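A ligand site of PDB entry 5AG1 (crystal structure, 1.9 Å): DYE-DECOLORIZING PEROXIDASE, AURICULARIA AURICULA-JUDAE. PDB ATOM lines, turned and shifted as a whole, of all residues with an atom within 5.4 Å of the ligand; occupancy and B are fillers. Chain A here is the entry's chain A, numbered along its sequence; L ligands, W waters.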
ATOM      1  N   GLU A 160       3.851  25.271  11.847  1.00  0.00           N
ATOM      2  CA  GLU A 160       2.606  25.983  12.124  1.00  0.00           C
ATOM      3  C   GLU A 160       2.306  25.962  13.621  1.00  0.00           C
ATOM      4  O   GLU A 160       3.123  25.498  14.409  1.00  0.00           O
ATOM      5  CB  GLU A 160       1.448  25.433  11.288  1.00  0.00           C
ATOM      6  CG  GLU A 160       1.250  23.934  11.384  1.00  0.00           C
ATOM      7  CD  GLU A 160       0.849  23.512  12.773  1.00  0.00           C
ATOM      8  OE1 GLU A 160      -0.245  23.911  13.228  1.00  0.00           O
ATOM      9  OE2 GLU A 160       1.640  22.795  13.429  1.00  0.00           O
ATOM     10  N   PHE A 162       0.443  24.497  15.753  1.00  0.00           N
ATOM     11  CA  PHE A 162       0.378  23.267  16.538  1.00  0.00           C
ATOM     12  C   PHE A 162       1.760  22.703  16.800  1.00  0.00           C
ATOM     13  O   PHE A 162       1.932  21.808  17.639  1.00  0.00           O
ATOM     14  CB  PHE A 162      -0.475  22.195  15.844  1.00  0.00           C
ATOM     15  CG  PHE A 162      -1.962  22.411  15.954  1.00  0.00           C
ATOM     16  CD1 PHE A 162      -2.513  23.025  17.072  1.00  0.00           C
ATOM     17  CD2 PHE A 162      -2.808  21.963  14.961  1.00  0.00           C
ATOM     18  CE1 PHE A 162      -3.872  23.238  17.157  1.00  0.00           C
ATOM     19  CE2 PHE A 162      -4.174  22.156  15.046  1.00  0.00           C
ATOM     20  CZ  PHE A 162      -4.710  22.797  16.154  1.00  0.00           C
ATOM     21  N   PHE A 164       3.923  21.628  14.094  1.00  0.00           N
ATOM     22  CA  PHE A 164       4.324  20.675  13.055  1.00  0.00           C
ATOM     23  C   PHE A 164       4.997  21.388  11.889  1.00  0.00           C
ATOM     24  O   PHE A 164       4.543  22.449  11.462  1.00  0.00           O
ATOM     25  CB  PHE A 164       3.114  19.891  12.556  1.00  0.00           C
ATOM     26  CG  PHE A 164       2.542  18.952  13.585  1.00  0.00           C
ATOM     27  CD1 PHE A 164       1.724  19.426  14.596  1.00  0.00           C
ATOM     28  CD2 PHE A 164       2.875  17.606  13.564  1.00  0.00           C
ATOM     29  CE1 PHE A 164       1.219  18.566  15.558  1.00  0.00           C
ATOM     30  CE2 PHE A 164       2.378  16.743  14.520  1.00  0.00           C
ATOM     31  CZ  PHE A 164       1.553  17.224  15.520  1.00  0.00           C
ATOM     32  N   LEU A 165       6.090  20.813  11.395  1.00  0.00           N
ATOM     33  CA  LEU A 165       6.726  21.307  10.184  1.00  0.00           C
ATOM     34  C   LEU A 165       5.724  21.273   9.027  1.00  0.00           C
ATOM     35  O   LEU A 165       5.051  20.270   8.812  1.00  0.00           O
ATOM     36  CB  LEU A 165       7.973  20.490   9.825  1.00  0.00           C
ATOM     37  CG  LEU A 165       8.855  21.040   8.698  1.00  0.00           C
ATOM     38  CD1 LEU A 165       9.510  22.354   9.112  1.00  0.00           C
ATOM     39  CD2 LEU A 165       9.915  20.022   8.304  1.00  0.00           C
ATOM     40  N   ASP A 166       5.672  22.374   8.288  1.00  0.00           N
ATOM     41  CA  ASP A 166       4.661  22.567   7.249  1.00  0.00           C
ATOM     42  C   ASP A 166       5.314  23.024   5.946  1.00  0.00           C
ATOM     43  O   ASP A 166       6.413  23.596   5.961  1.00  0.00           O
ATOM     44  CB  ASP A 166       3.633  23.602   7.721  1.00  0.00           C
ATOM     45  CG  ASP A 166       2.455  23.717   6.775  1.00  0.00           C
ATOM     46  OD1 ASP A 166       2.290  22.818   5.916  1.00  0.00           O
ATOM     47  OD2 ASP A 166       1.702  24.704   6.888  1.00  0.00           O
ATOM     48  N   GLY A 167       4.647  22.759   4.828  1.00  0.00           N
ATOM     49  CA  GLY A 167       5.220  23.070   3.525  1.00  0.00           C
ATOM     50  C   GLY A 167       6.220  22.039   3.035  1.00  0.00           C
ATOM     51  O   GLY A 167       7.126  22.362   2.268  1.00  0.00           O
ATOM     52  N   ILE A 168       6.049  20.791   3.453  1.00  0.00           N
ATOM     53  CA  ILE A 168       6.839  19.696   2.920  1.00  0.00           C
ATOM     54  C   ILE A 168       6.283  19.233   1.571  1.00  0.00           C
ATOM     55  O   ILE A 168       7.032  19.040   0.617  1.00  0.00           O
ATOM     56  CB  ILE A 168       6.852  18.488   3.881  1.00  0.00           C
ATOM     57  CG1 ILE A 168       7.485  18.882   5.220  1.00  0.00           C
ATOM     58  CG2 ILE A 168       7.573  17.308   3.257  1.00  0.00           C
ATOM     59  CD1 ILE A 168       7.163  17.931   6.352  1.00  0.00           C
ATOM     60  N   ALA A 169       4.972  19.039   1.518  1.00  0.00           N
ATOM     61  CA  ALA A 169       4.340  18.344   0.399  1.00  0.00           C
ATOM     62  C   ALA A 169       3.636  19.322  -0.550  1.00  0.00           C
ATOM     63  O   ALA A 169       2.804  20.107  -0.128  1.00  0.00           O
ATOM     64  CB  ALA A 169       3.355  17.307   0.913  1.00  0.00           C
ATOM     65  N   GLN A 170       4.018  19.273  -1.828  1.00  0.00           N
ATOM     66  CA  GLN A 170       3.314  20.012  -2.868  1.00  0.00           C
ATOM     67  C   GLN A 170       3.307  19.162  -4.119  1.00  0.00           C
ATOM     68  O   GLN A 170       4.200  18.334  -4.311  1.00  0.00           O
ATOM     69  CB  GLN A 170       4.040  21.332  -3.166  1.00  0.00           C
ATOM     70  CG  GLN A 170       4.388  22.171  -1.945  1.00  0.00           C
ATOM     71  CD  GLN A 170       3.254  23.092  -1.531  1.00  0.00           C
ATOM     72  OE1 GLN A 170       2.116  22.942  -1.989  1.00  0.00           O
ATOM     73  NE2 GLN A 170       3.552  24.039  -0.648  1.00  0.00           N
ATOM     74  N   LEU A 217      -8.095  30.319   9.569  1.00  0.00           N
ATOM     75  CA  LEU A 217      -8.373  29.146  10.401  1.00  0.00           C
ATOM     76  C   LEU A 217      -7.746  29.286  11.777  1.00  0.00           C
ATOM     77  O   LEU A 217      -6.538  29.085  11.939  1.00  0.00           O
ATOM     78  CB  LEU A 217      -7.857  27.880   9.704  1.00  0.00           C
ATOM     79  CG  LEU A 217      -8.472  27.604   8.336  1.00  0.00           C
ATOM     80  CD1 LEU A 217      -7.910  26.328   7.728  1.00  0.00           C
ATOM     81  CD2 LEU A 217      -9.991  27.542   8.415  1.00  0.00           C
ATOM     82  N   GLN A 219      -6.558  28.294  15.344  1.00  0.00           N
ATOM     83  CA  GLN A 219      -6.143  27.045  15.978  1.00  0.00           C
ATOM     84  C   GLN A 219      -6.172  27.180  17.485  1.00  0.00           C
ATOM     85  O   GLN A 219      -5.641  28.137  18.047  1.00  0.00           O
ATOM     86  CB  GLN A 219      -4.743  26.656  15.492  1.00  0.00           C
ATOM     87  CG  GLN A 219      -4.697  26.288  14.021  1.00  0.00           C
ATOM     88  CD  GLN A 219      -3.286  26.104  13.510  1.00  0.00           C
ATOM     89  OE1 GLN A 219      -2.756  26.962  12.799  1.00  0.00           O
ATOM     90  NE2 GLN A 219      -2.667  24.989  13.865  1.00  0.00           N
ATOM     91  N   VAL A 251      -2.111  13.978  12.540  1.00  0.00           N
ATOM     92  CA  VAL A 251      -1.588  14.773  11.437  1.00  0.00           C
ATOM     93  C   VAL A 251      -1.125  13.873  10.289  1.00  0.00           C
ATOM     94  O   VAL A 251      -1.393  14.163   9.117  1.00  0.00           O
ATOM     95  CB  VAL A 251      -0.410  15.663  11.901  1.00  0.00           C
ATOM     96  CG1 VAL A 251       0.250  16.342  10.703  1.00  0.00           C
ATOM     97  CG2 VAL A 251      -0.886  16.695  12.915  1.00  0.00           C
ATOM     98  N   ARG A 253       2.147  13.176  10.300  1.00  0.00           N
ATOM     99  CA  ARG A 253       3.583  13.441  10.436  1.00  0.00           C
ATOM    100  C   ARG A 253       3.907  13.788  11.882  1.00  0.00           C
ATOM    101  O   ARG A 253       3.059  14.340  12.590  1.00  0.00           O
ATOM    102  CB  ARG A 253       4.005  14.605   9.537  1.00  0.00           C
ATOM    103  CG  ARG A 253       3.813  14.387   8.046  1.00  0.00           C
ATOM    104  CD  ARG A 253       4.436  15.515   7.236  1.00  0.00           C
ATOM    105  NE  ARG A 253       4.325  15.254   5.809  1.00  0.00           N
ATOM    106  CZ  ARG A 253       5.220  14.581   5.097  1.00  0.00           C
ATOM    107  NH1 ARG A 253       6.323  14.123   5.671  1.00  0.00           N
ATOM    108  NH2 ARG A 253       5.013  14.360   3.796  1.00  0.00           N
ATOM    109  N   ASN A 279       9.018  12.467   1.986  1.00  0.00           N
ATOM    110  CA  ASN A 279       7.785  12.285   1.212  1.00  0.00           C
ATOM    111  C   ASN A 279       7.769  11.002   0.398  1.00  0.00           C
ATOM    112  O   ASN A 279       6.870  10.765  -0.412  1.00  0.00           O
ATOM    113  CB  ASN A 279       7.529  13.495   0.318  1.00  0.00           C
ATOM    114  CG  ASN A 279       6.053  13.804   0.166  1.00  0.00           C
ATOM    115  OD1 ASN A 279       5.242  13.434   1.015  1.00  0.00           O
ATOM    116  ND2 ASN A 279       5.697  14.482  -0.922  1.00  0.00           N
ATOM    117  N   TYR A 283       1.850   4.743   1.498  1.00  0.00           N
ATOM    118  CA  TYR A 283       0.959   4.090   2.467  1.00  0.00           C
ATOM    119  C   TYR A 283       0.926   2.569   2.349  1.00  0.00           C
ATOM    120  O   TYR A 283       0.364   1.885   3.205  1.00  0.00           O
ATOM    121  CB  TYR A 283      -0.459   4.684   2.420  1.00  0.00           C
ATOM    122  CG  TYR A 283      -0.509   6.133   2.850  1.00  0.00           C
ATOM    123  CD1 TYR A 283       0.051   6.541   4.053  1.00  0.00           C
ATOM    124  CD2 TYR A 283      -1.070   7.099   2.024  1.00  0.00           C
ATOM    125  CE1 TYR A 283       0.051   7.873   4.431  1.00  0.00           C
ATOM    126  CE2 TYR A 283      -1.085   8.431   2.401  1.00  0.00           C
ATOM    127  CZ  TYR A 283      -0.524   8.816   3.598  1.00  0.00           C
ATOM    128  OH  TYR A 283      -0.532  10.136   3.973  1.00  0.00           O
ATOM    129  N   HIS A 302      -4.659  13.574   8.793  1.00  0.00           N
ATOM    130  CA  HIS A 302      -4.811  14.770   7.931  1.00  0.00           C
ATOM    131  C   HIS A 302      -4.221  14.562   6.530  1.00  0.00           C
ATOM    132  O   HIS A 302      -4.916  14.720   5.538  1.00  0.00           O
ATOM    133  CB  HIS A 302      -4.201  16.018   8.588  1.00  0.00           C
ATOM    134  CG  HIS A 302      -4.204  17.262   7.720  1.00  0.00           C
ATOM    135  ND1 HIS A 302      -5.356  17.790   7.185  1.00  0.00           N
ATOM    136  CD2 HIS A 302      -3.216  18.139   7.433  1.00  0.00           C
ATOM    137  CE1 HIS A 302      -5.066  18.909   6.548  1.00  0.00           C
ATOM    138  NE2 HIS A 302      -3.779  19.154   6.679  1.00  0.00           N
ATOM    139  N   ILE A 303      -2.928  14.249   6.458  1.00  0.00           N
ATOM    140  CA  ILE A 303      -2.276  14.181   5.151  1.00  0.00           C
ATOM    141  C   ILE A 303      -2.770  13.022   4.289  1.00  0.00           C
ATOM    142  O   ILE A 303      -2.749  13.101   3.063  1.00  0.00           O
ATOM    143  CB  ILE A 303      -0.737  14.180   5.248  1.00  0.00           C
ATOM    144  CG1 ILE A 303      -0.218  12.905   5.933  1.00  0.00           C
ATOM    145  CG2 ILE A 303      -0.235  15.438   5.951  1.00  0.00           C
ATOM    146  CD1 ILE A 303       1.240  12.631   5.640  1.00  0.00           C
ATOM    147  N   THR A 306      -6.075  14.193   2.763  1.00  0.00           N
ATOM    148  CA  THR A 306      -5.955  15.254   1.764  1.00  0.00           C
ATOM    149  C   THR A 306      -5.106  14.876   0.559  1.00  0.00           C
ATOM    150  O   THR A 306      -5.238  15.481  -0.509  1.00  0.00           O
ATOM    151  CB  THR A 306      -5.448  16.571   2.369  1.00  0.00           C
ATOM    152  OG1 THR A 306      -4.204  16.340   3.044  1.00  0.00           O
ATOM    153  CG2 THR A 306      -6.469  17.121   3.367  1.00  0.00           C
ATOM    154  N   ARG A 307      -4.208  13.908   0.731  1.00  0.00           N
ATOM    155  CA  ARG A 307      -3.595  13.201  -0.403  1.00  0.00           C
ATOM    156  C   ARG A 307      -3.551  11.695  -0.137  1.00  0.00           C
ATOM    157  O   ARG A 307      -2.667  11.206   0.563  1.00  0.00           O
ATOM    158  CB  ARG A 307      -2.200  13.731  -0.725  1.00  0.00           C
ATOM    159  CG  ARG A 307      -1.621  13.167  -2.020  1.00  0.00           C
ATOM    160  CD  ARG A 307      -0.102  13.229  -2.099  1.00  0.00           C
ATOM    161  NE  ARG A 307       0.396  12.397  -3.204  1.00  0.00           N
ATOM    162  CZ  ARG A 307       1.672  12.060  -3.396  1.00  0.00           C
ATOM    163  NH1 ARG A 307       2.626  12.567  -2.634  1.00  0.00           N
ATOM    164  NH2 ARG A 307       1.995  11.243  -4.391  1.00  0.00           N
ATOM    165  N   ARG A 309      -2.918   9.045  -1.847  1.00  0.00           N
ATOM    166  CA  ARG A 309      -1.922   8.195  -2.481  1.00  0.00           C
ATOM    167  C   ARG A 309      -2.489   6.821  -2.847  1.00  0.00           C
ATOM    168  O   ARG A 309      -3.503   6.734  -3.552  1.00  0.00           O
ATOM    169  CB  ARG A 309      -0.656   8.100  -1.615  1.00  0.00           C
ATOM    170  CG  ARG A 309      -0.126   9.468  -1.211  1.00  0.00           C
ATOM    171  CD  ARG A 309       1.194   9.424  -0.431  1.00  0.00           C
ATOM    172  NE  ARG A 309       1.460  10.736   0.169  1.00  0.00           N
ATOM    173  CZ  ARG A 309       2.661  11.296   0.275  1.00  0.00           C
ATOM    174  NH1 ARG A 309       3.750  10.657  -0.134  1.00  0.00           N
ATOM    175  NH2 ARG A 309       2.773  12.499   0.804  1.00  0.00           N
ATOM    176  N   ILE A 328      -3.593  20.585  -4.627  1.00  0.00           N
ATOM    177  CA  ILE A 328      -3.529  22.035  -4.413  1.00  0.00           C
ATOM    178  C   ILE A 328      -2.091  22.452  -4.100  1.00  0.00           C
ATOM    179  O   ILE A 328      -1.334  21.689  -3.511  1.00  0.00           O
ATOM    180  CB  ILE A 328      -4.425  22.476  -3.241  1.00  0.00           C
ATOM    181  CG1 ILE A 328      -4.048  21.708  -1.966  1.00  0.00           C
ATOM    182  CG2 ILE A 328      -5.894  22.240  -3.586  1.00  0.00           C
ATOM    183  CD1 ILE A 328      -4.719  22.237  -0.714  1.00  0.00           C
ATOM    184  N   ARG A 330      -0.067  24.870  -1.684  1.00  0.00           N
ATOM    185  CA  ARG A 330      -0.334  25.519  -0.396  1.00  0.00           C
ATOM    186  C   ARG A 330       0.684  26.614  -0.106  1.00  0.00           C
ATOM    187  O   ARG A 330       1.893  26.373  -0.163  1.00  0.00           O
ATOM    188  CB  ARG A 330      -0.345  24.491   0.730  1.00  0.00           C
ATOM    189  CG  ARG A 330      -1.584  23.605   0.747  1.00  0.00           C
ATOM    190  CD  ARG A 330      -1.473  22.496   1.779  1.00  0.00           C
ATOM    191  NE  ARG A 330      -0.226  21.747   1.629  1.00  0.00           N
ATOM    192  CZ  ARG A 330       0.661  21.583   2.592  1.00  0.00           C
ATOM    193  NH1 ARG A 330       0.444  22.070   3.800  1.00  0.00           N
ATOM    194  NH2 ARG A 330       1.792  20.931   2.349  1.00  0.00           N
ATOM    195  N   LEU A 355      -3.758  29.679  11.305  1.00  0.00           N
ATOM    196  CA  LEU A 355      -3.148  29.573   9.980  1.00  0.00           C
ATOM    197  C   LEU A 355      -3.909  30.457   9.005  1.00  0.00           C
ATOM    198  O   LEU A 355      -5.130  30.330   8.853  1.00  0.00           O
ATOM    199  CB  LEU A 355      -3.166  28.129   9.501  1.00  0.00           C
ATOM    200  CG  LEU A 355      -2.502  27.852   8.152  1.00  0.00           C
ATOM    201  CD1 LEU A 355      -0.996  28.044   8.273  1.00  0.00           C
ATOM    202  CD2 LEU A 355      -2.823  26.457   7.666  1.00  0.00           C
ATOM    203  N   PHE A 357      -4.640  30.319   5.769  1.00  0.00           N
ATOM    204  CA  PHE A 357      -4.563  29.225   4.811  1.00  0.00           C
ATOM    205  C   PHE A 357      -4.733  29.753   3.400  1.00  0.00           C
ATOM    206  O   PHE A 357      -5.651  30.524   3.129  1.00  0.00           O
ATOM    207  CB  PHE A 357      -5.626  28.175   5.116  1.00  0.00           C
ATOM    208  CG  PHE A 357      -5.662  27.034   4.141  1.00  0.00           C
ATOM    209  CD1 PHE A 357      -4.874  25.911   4.346  1.00  0.00           C
ATOM    210  CD2 PHE A 357      -6.496  27.070   3.040  1.00  0.00           C
ATOM    211  CE1 PHE A 357      -4.898  24.861   3.443  1.00  0.00           C
ATOM    212  CE2 PHE A 357      -6.548  26.017   2.153  1.00  0.00           C
ATOM    213  CZ  PHE A 357      -5.746  24.911   2.351  1.00  0.00           C
ATOM    214  N   PHE A 368      -9.422  22.719  -3.121  1.00  0.00           N
ATOM    215  CA  PHE A 368      -9.722  22.953  -1.714  1.00  0.00           C
ATOM    216  C   PHE A 368     -11.117  22.476  -1.336  1.00  0.00           C
ATOM    217  O   PHE A 368     -11.302  21.755  -0.348  1.00  0.00           O
ATOM    218  CB  PHE A 368      -9.549  24.432  -1.356  1.00  0.00           C
ATOM    219  CG  PHE A 368     -10.313  24.838  -0.128  1.00  0.00           C
ATOM    220  CD1 PHE A 368      -9.873  24.478   1.129  1.00  0.00           C
ATOM    221  CD2 PHE A 368     -11.530  25.497  -0.238  1.00  0.00           C
ATOM    222  CE1 PHE A 368     -10.592  24.814   2.264  1.00  0.00           C
ATOM    223  CE2 PHE A 368     -12.255  25.849   0.883  1.00  0.00           C
ATOM    224  CZ  PHE A 368     -11.786  25.499   2.138  1.00  0.00           C
ATOM    225  N   LEU A 371     -11.339  18.633  -1.385  1.00  0.00           N
ATOM    226  CA  LEU A 371     -10.600  18.062  -0.264  1.00  0.00           C
ATOM    227  C   LEU A 371     -11.350  18.222   1.051  1.00  0.00           C
ATOM    228  O   LEU A 371     -11.404  17.292   1.866  1.00  0.00           O
ATOM    229  CB  LEU A 371      -9.207  18.702  -0.159  1.00  0.00           C
ATOM    230  CG  LEU A 371      -8.051  17.988  -0.870  1.00  0.00           C
ATOM    231  CD1 LEU A 371      -8.433  17.600  -2.287  1.00  0.00           C
ATOM    232  CD2 LEU A 371      -6.791  18.853  -0.885  1.00  0.00           C
ATOM    233  N   GLN A 372     -11.927  19.404   1.270  1.00  0.00           N
ATOM    234  CA  GLN A 372     -12.637  19.662   2.510  1.00  0.00           C
ATOM    235  C   GLN A 372     -13.935  18.849   2.603  1.00  0.00           C
ATOM    236  O   GLN A 372     -14.183  18.189   3.604  1.00  0.00           O
ATOM    237  CB  GLN A 372     -12.938  21.154   2.666  1.00  0.00           C
ATOM    238  CG  GLN A 372     -13.683  21.511   3.936  1.00  0.00           C
ATOM    239  CD  GLN A 372     -12.806  21.452   5.176  1.00  0.00           C
ATOM    240  OE1 GLN A 372     -11.793  22.154   5.276  1.00  0.00           O
ATOM    241  NE2 GLN A 372     -13.161  20.577   6.111  1.00  0.00           N
ATOM    242  N   ILE A 395      -8.017  17.086  12.097  1.00  0.00           N
ATOM    243  CA  ILE A 395      -7.477  18.446  12.058  1.00  0.00           C
ATOM    244  C   ILE A 395      -8.471  19.434  11.451  1.00  0.00           C
ATOM    245  O   ILE A 395      -8.762  20.467  12.062  1.00  0.00           O
ATOM    246  CB  ILE A 395      -6.130  18.504  11.308  1.00  0.00           C
ATOM    247  CG1 ILE A 395      -5.109  17.564  11.958  1.00  0.00           C
ATOM    248  CG2 ILE A 395      -5.596  19.932  11.251  1.00  0.00           C
ATOM    249  CD1 ILE A 395      -4.808  17.881  13.407  1.00  0.00           C
ATOM    250  N   ILE A 396      -9.010  19.123  10.280  1.00  0.00           N
ATOM    251  CA  ILE A 396      -9.887  20.074   9.585  1.00  0.00           C
ATOM    252  C   ILE A 396     -11.317  19.570   9.381  1.00  0.00           C
ATOM    253  O   ILE A 396     -12.164  20.308   8.890  1.00  0.00           O
ATOM    254  CB  ILE A 396      -9.310  20.515   8.232  1.00  0.00           C
ATOM    255  CG1 ILE A 396      -9.144  19.318   7.293  1.00  0.00           C
ATOM    256  CG2 ILE A 396      -8.004  21.257   8.432  1.00  0.00           C
ATOM    257  CD1 ILE A 396      -9.066  19.702   5.832  1.00  0.00           C
ATOM    258  N   VAL A 424      -9.623  23.392  15.180  1.00  0.00           N
ATOM    259  CA  VAL A 424      -9.510  24.423  14.155  1.00  0.00           C
ATOM    260  C   VAL A 424     -10.892  25.039  13.920  1.00  0.00           C
ATOM    261  O   VAL A 424     -11.864  24.322  13.699  1.00  0.00           O
ATOM    262  CB  VAL A 424      -9.014  23.826  12.824  1.00  0.00           C
ATOM    263  CG1 VAL A 424      -9.046  24.878  11.733  1.00  0.00           C
ATOM    264  CG2 VAL A 424      -7.607  23.281  12.996  1.00  0.00           C
HETATM  265 FE1  LIG L   1      -3.059  20.737   5.948  1.00  0.00          FE
HETATM  266  N1  LIG L   1      -1.217  20.809  10.396  1.00  0.00           N
HETATM  267  O1  LIG L   1      -1.722  19.695  11.084  1.00  0.00           O
HETATM  268  O2  LIG L   1      -0.461  21.602  10.937  1.00  0.00           O
HETATM  269  N2  LIG L   1      -1.369  20.104   6.784  1.00  0.00           N
HETATM  270  N3  LIG L   1      -3.528  21.817   7.679  1.00  0.00           N
HETATM  271  N4  LIG L   1      -4.827  21.421   5.098  1.00  0.00           N
HETATM  272  N5  LIG L   1      -2.637  19.789   4.363  1.00  0.00           N
HETATM  273  C1  LIG L   1      -0.371  19.400   6.139  1.00  0.00           C
HETATM  274  O3  LIG L   1       3.025  17.829   4.284  1.00  0.00           O
HETATM  275  C2  LIG L   1      -2.800  21.852   8.787  1.00  0.00           C
HETATM  276  C3  LIG L   1      -5.704  22.324   5.626  1.00  0.00           C
HETATM  277  C4  LIG L   1      -3.379  19.726   3.234  1.00  0.00           C
HETATM  278  O4  LIG L   1       0.612  14.471   1.479  1.00  0.00           O
HETATM  279  C5  LIG L   1       0.679  19.149   7.057  1.00  0.00           C
HETATM  280  O5  LIG L   1       3.630  19.874   3.941  1.00  0.00           O
HETATM  281  C6  LIG L   1      -3.395  22.750   9.720  1.00  0.00           C
HETATM  282  C7  LIG L   1      -6.800  22.454   4.752  1.00  0.00           C
HETATM  283  C8  LIG L   1      -2.676  18.988   2.168  1.00  0.00           C
HETATM  284  O6  LIG L   1       0.493  15.914  -0.112  1.00  0.00           O
HETATM  285  C9  LIG L   1       0.344  19.715   8.238  1.00  0.00           C
HETATM  286  C10 LIG L   1      -4.495  23.301   9.110  1.00  0.00           C
HETATM  287  C11 LIG L   1      -6.550  21.643   3.654  1.00  0.00           C
HETATM  288  C12 LIG L   1      -1.485  18.631   2.677  1.00  0.00           C
HETATM  289  C13 LIG L   1      -0.913  20.341   8.064  1.00  0.00           C
HETATM  290  C14 LIG L   1      -4.543  22.692   7.758  1.00  0.00           C
HETATM  291  C15 LIG L   1      -5.295  21.004   3.879  1.00  0.00           C
HETATM  292  C16 LIG L   1      -1.459  19.191   4.039  1.00  0.00           C
HETATM  293  C17 LIG L   1       1.938  18.375   6.758  1.00  0.00           C
HETATM  294  C18 LIG L   1      -5.440  24.308   9.625  1.00  0.00           C
HETATM  295  C19 LIG L   1      -7.384  21.426   2.452  1.00  0.00           C
HETATM  296  C20 LIG L   1      -0.393  17.855   1.965  1.00  0.00           C
HETATM  297  C21 LIG L   1       2.982  19.315   6.162  1.00  0.00           C
HETATM  298  C22 LIG L   1      -5.076  25.269  10.467  1.00  0.00           C
HETATM  299  C23 LIG L   1      -8.690  21.606   2.454  1.00  0.00           C
HETATM  300  C24 LIG L   1      -0.775  16.363   1.893  1.00  0.00           C
HETATM  301  C25 LIG L   1       3.218  18.979   4.708  1.00  0.00           C
HETATM  302  C26 LIG L   1       0.179  15.553   1.052  1.00  0.00           C
HETATM  303  C27 LIG L   1      -0.355  18.982   4.845  1.00  0.00           C
HETATM  304  C28 LIG L   1      -1.593  21.013   9.072  1.00  0.00           C
HETATM  305  C29 LIG L   1      -5.557  22.987   6.847  1.00  0.00           C
HETATM  306  C30 LIG L   1      -4.680  20.162   3.009  1.00  0.00           C
HETATM  307  C31 LIG L   1       1.172  19.708   9.495  1.00  0.00           C
HETATM  308  C32 LIG L   1      -2.915  23.055  11.126  1.00  0.00           C
HETATM  309  C33 LIG L   1      -8.004  23.354   4.967  1.00  0.00           C
HETATM  310  C34 LIG L   1      -3.201  18.665   0.798  1.00  0.00           C
HETATM  311  O   HOH W   1       2.759  15.017  -1.413  1.00  0.00           O
HETATM  312  O   HOH W   2      -0.445  11.909   1.944  1.00  0.00           O
HETATM  313  O   HOH W   3       2.444  15.270   3.447  1.00  0.00           O
HETATM  314  O   HOH W   4      -0.034  18.101  -1.835  1.00  0.00           O
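O of His 302 sits at hydrogen-bond distance from OG1 of Thr 306, 3.1 Å away. The backbone carbonyl oxygen (O) of Val 251 is in hydrogen-bond range of the backbone NH (N) of His 302, at 3.3 Å. The backbone carbonyl oxygen (O) of Arg 330 lies within hydrogen-bond range of the side-chain amide nitrogen (NE2) of Gln 170 (2.9 Å). The backbone NH (N) of Phe 164 is in hydrogen-bond range of the side-chain carboxylate (OE2) of Glu 160, 2.6 Å away. NH2 of Arg 253 sits at hydrogen-bond distance from OD1 of Asn 279 (2.9 Å). The backbone NH of Leu 355 is in hydrogen-bond range of the side-chain amide oxygen of Gln 219 (3.3 Å). NE2 of Gln 372 sits at hydrogen-bond distance from O of Ile 396 (3.0 Å). The backbone carbonyl oxygen of Leu 217 lies within hydrogen-bond range of the backbone NH of Leu 355, 2.9 Å away.
FE1 of the ligand is bound by NE2 of His 302 (1.9 Å). The backbone NH (N) of Ile 168 lies within hydrogen-bond range of an oxygen (O5) of the ligand (2.6 Å). NH2 of Arg 330 is in salt-bridge range of O5 of the ligand. An oxygen (O5) of the ligand sits at hydrogen-bond distance from the backbone NH of Ala 169 (2.9 Å). The guanidinium group (NH2) of Arg 309 is in salt-bridge range of an oxygen (O4) of the ligand (3.0 Å). An oxygen (O5) of the ligand sits at hydrogen-bond distance from the backbone NH (N) of Gly 167. The guanidinium group of Arg 253 is in salt-bridge range of an oxygen (O3) of the ligand.
The side-chain carboxylate of Glu 160 lies close to an oxygen (O2) of the ligand (3.3 Å). Phe 162 touches the ligand. CB of Phe 164 touches C31 of the ligand, 3.6 Å away. Leu 165 touches the ligand. OD1 of Asp 166 touches C21 of the ligand (3.6 Å). CD1 of Leu 217 touches C18 of the ligand (3.7 Å). Gln 219 touches the ligand (NE2 to C32, 3.4 Å). Val 251 touches the ligand (CG2 to O1, 3.6 Å). Ile 303 touches the ligand (CG2 to C27, 3.7 Å). OG1 of Thr 306 touches C8 of the ligand, at 3.2 Å. CD of Arg 307 touches O6 of the ligand, 3.4 Å away. CB of Leu 355 touches C22 of the ligand, 3.6 Å away. Phe 357 touches the ligand (CE1 to C7, 3.3 Å). Phe 368 touches the ligand (CD1 to C23, 3.4 Å). CB of Leu 371 touches C23 of the ligand, at 3.9 Å. OE1 of Gln 372 touches C33 of the ligand (3.99 Å). Ile 395 touches the ligand. CG2 of Ile 396 touches C29 of the ligand (3.4 Å). Hydrophobic or aromatic side chains within 4 Å of the ligand: Phe 162, Phe 164, Ile 168, Ala 169, Leu 217, Val 251, His 302, Ile 303, Leu 355, Phe 357, Phe 368, Leu 371, Ile 395 and Ile 396.
Water W3 bridges the guanidinium group (NH2) of Arg 253 and an oxygen (O3) of the ligand. Water W2 lies within hydrogen-bond range of the side-chain hydroxyl (OH) of Tyr 283 (2.7 Å), the backbone carbonyl oxygen (O) of Arg 307 (2.7 Å), an oxygen (O4) of the ligand (2.8 Å), the backbone carbonyl oxygen (O) of Ile 303 (2.8 Å) and the guanidinium group (NE) of Arg 309 (2.9 Å).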
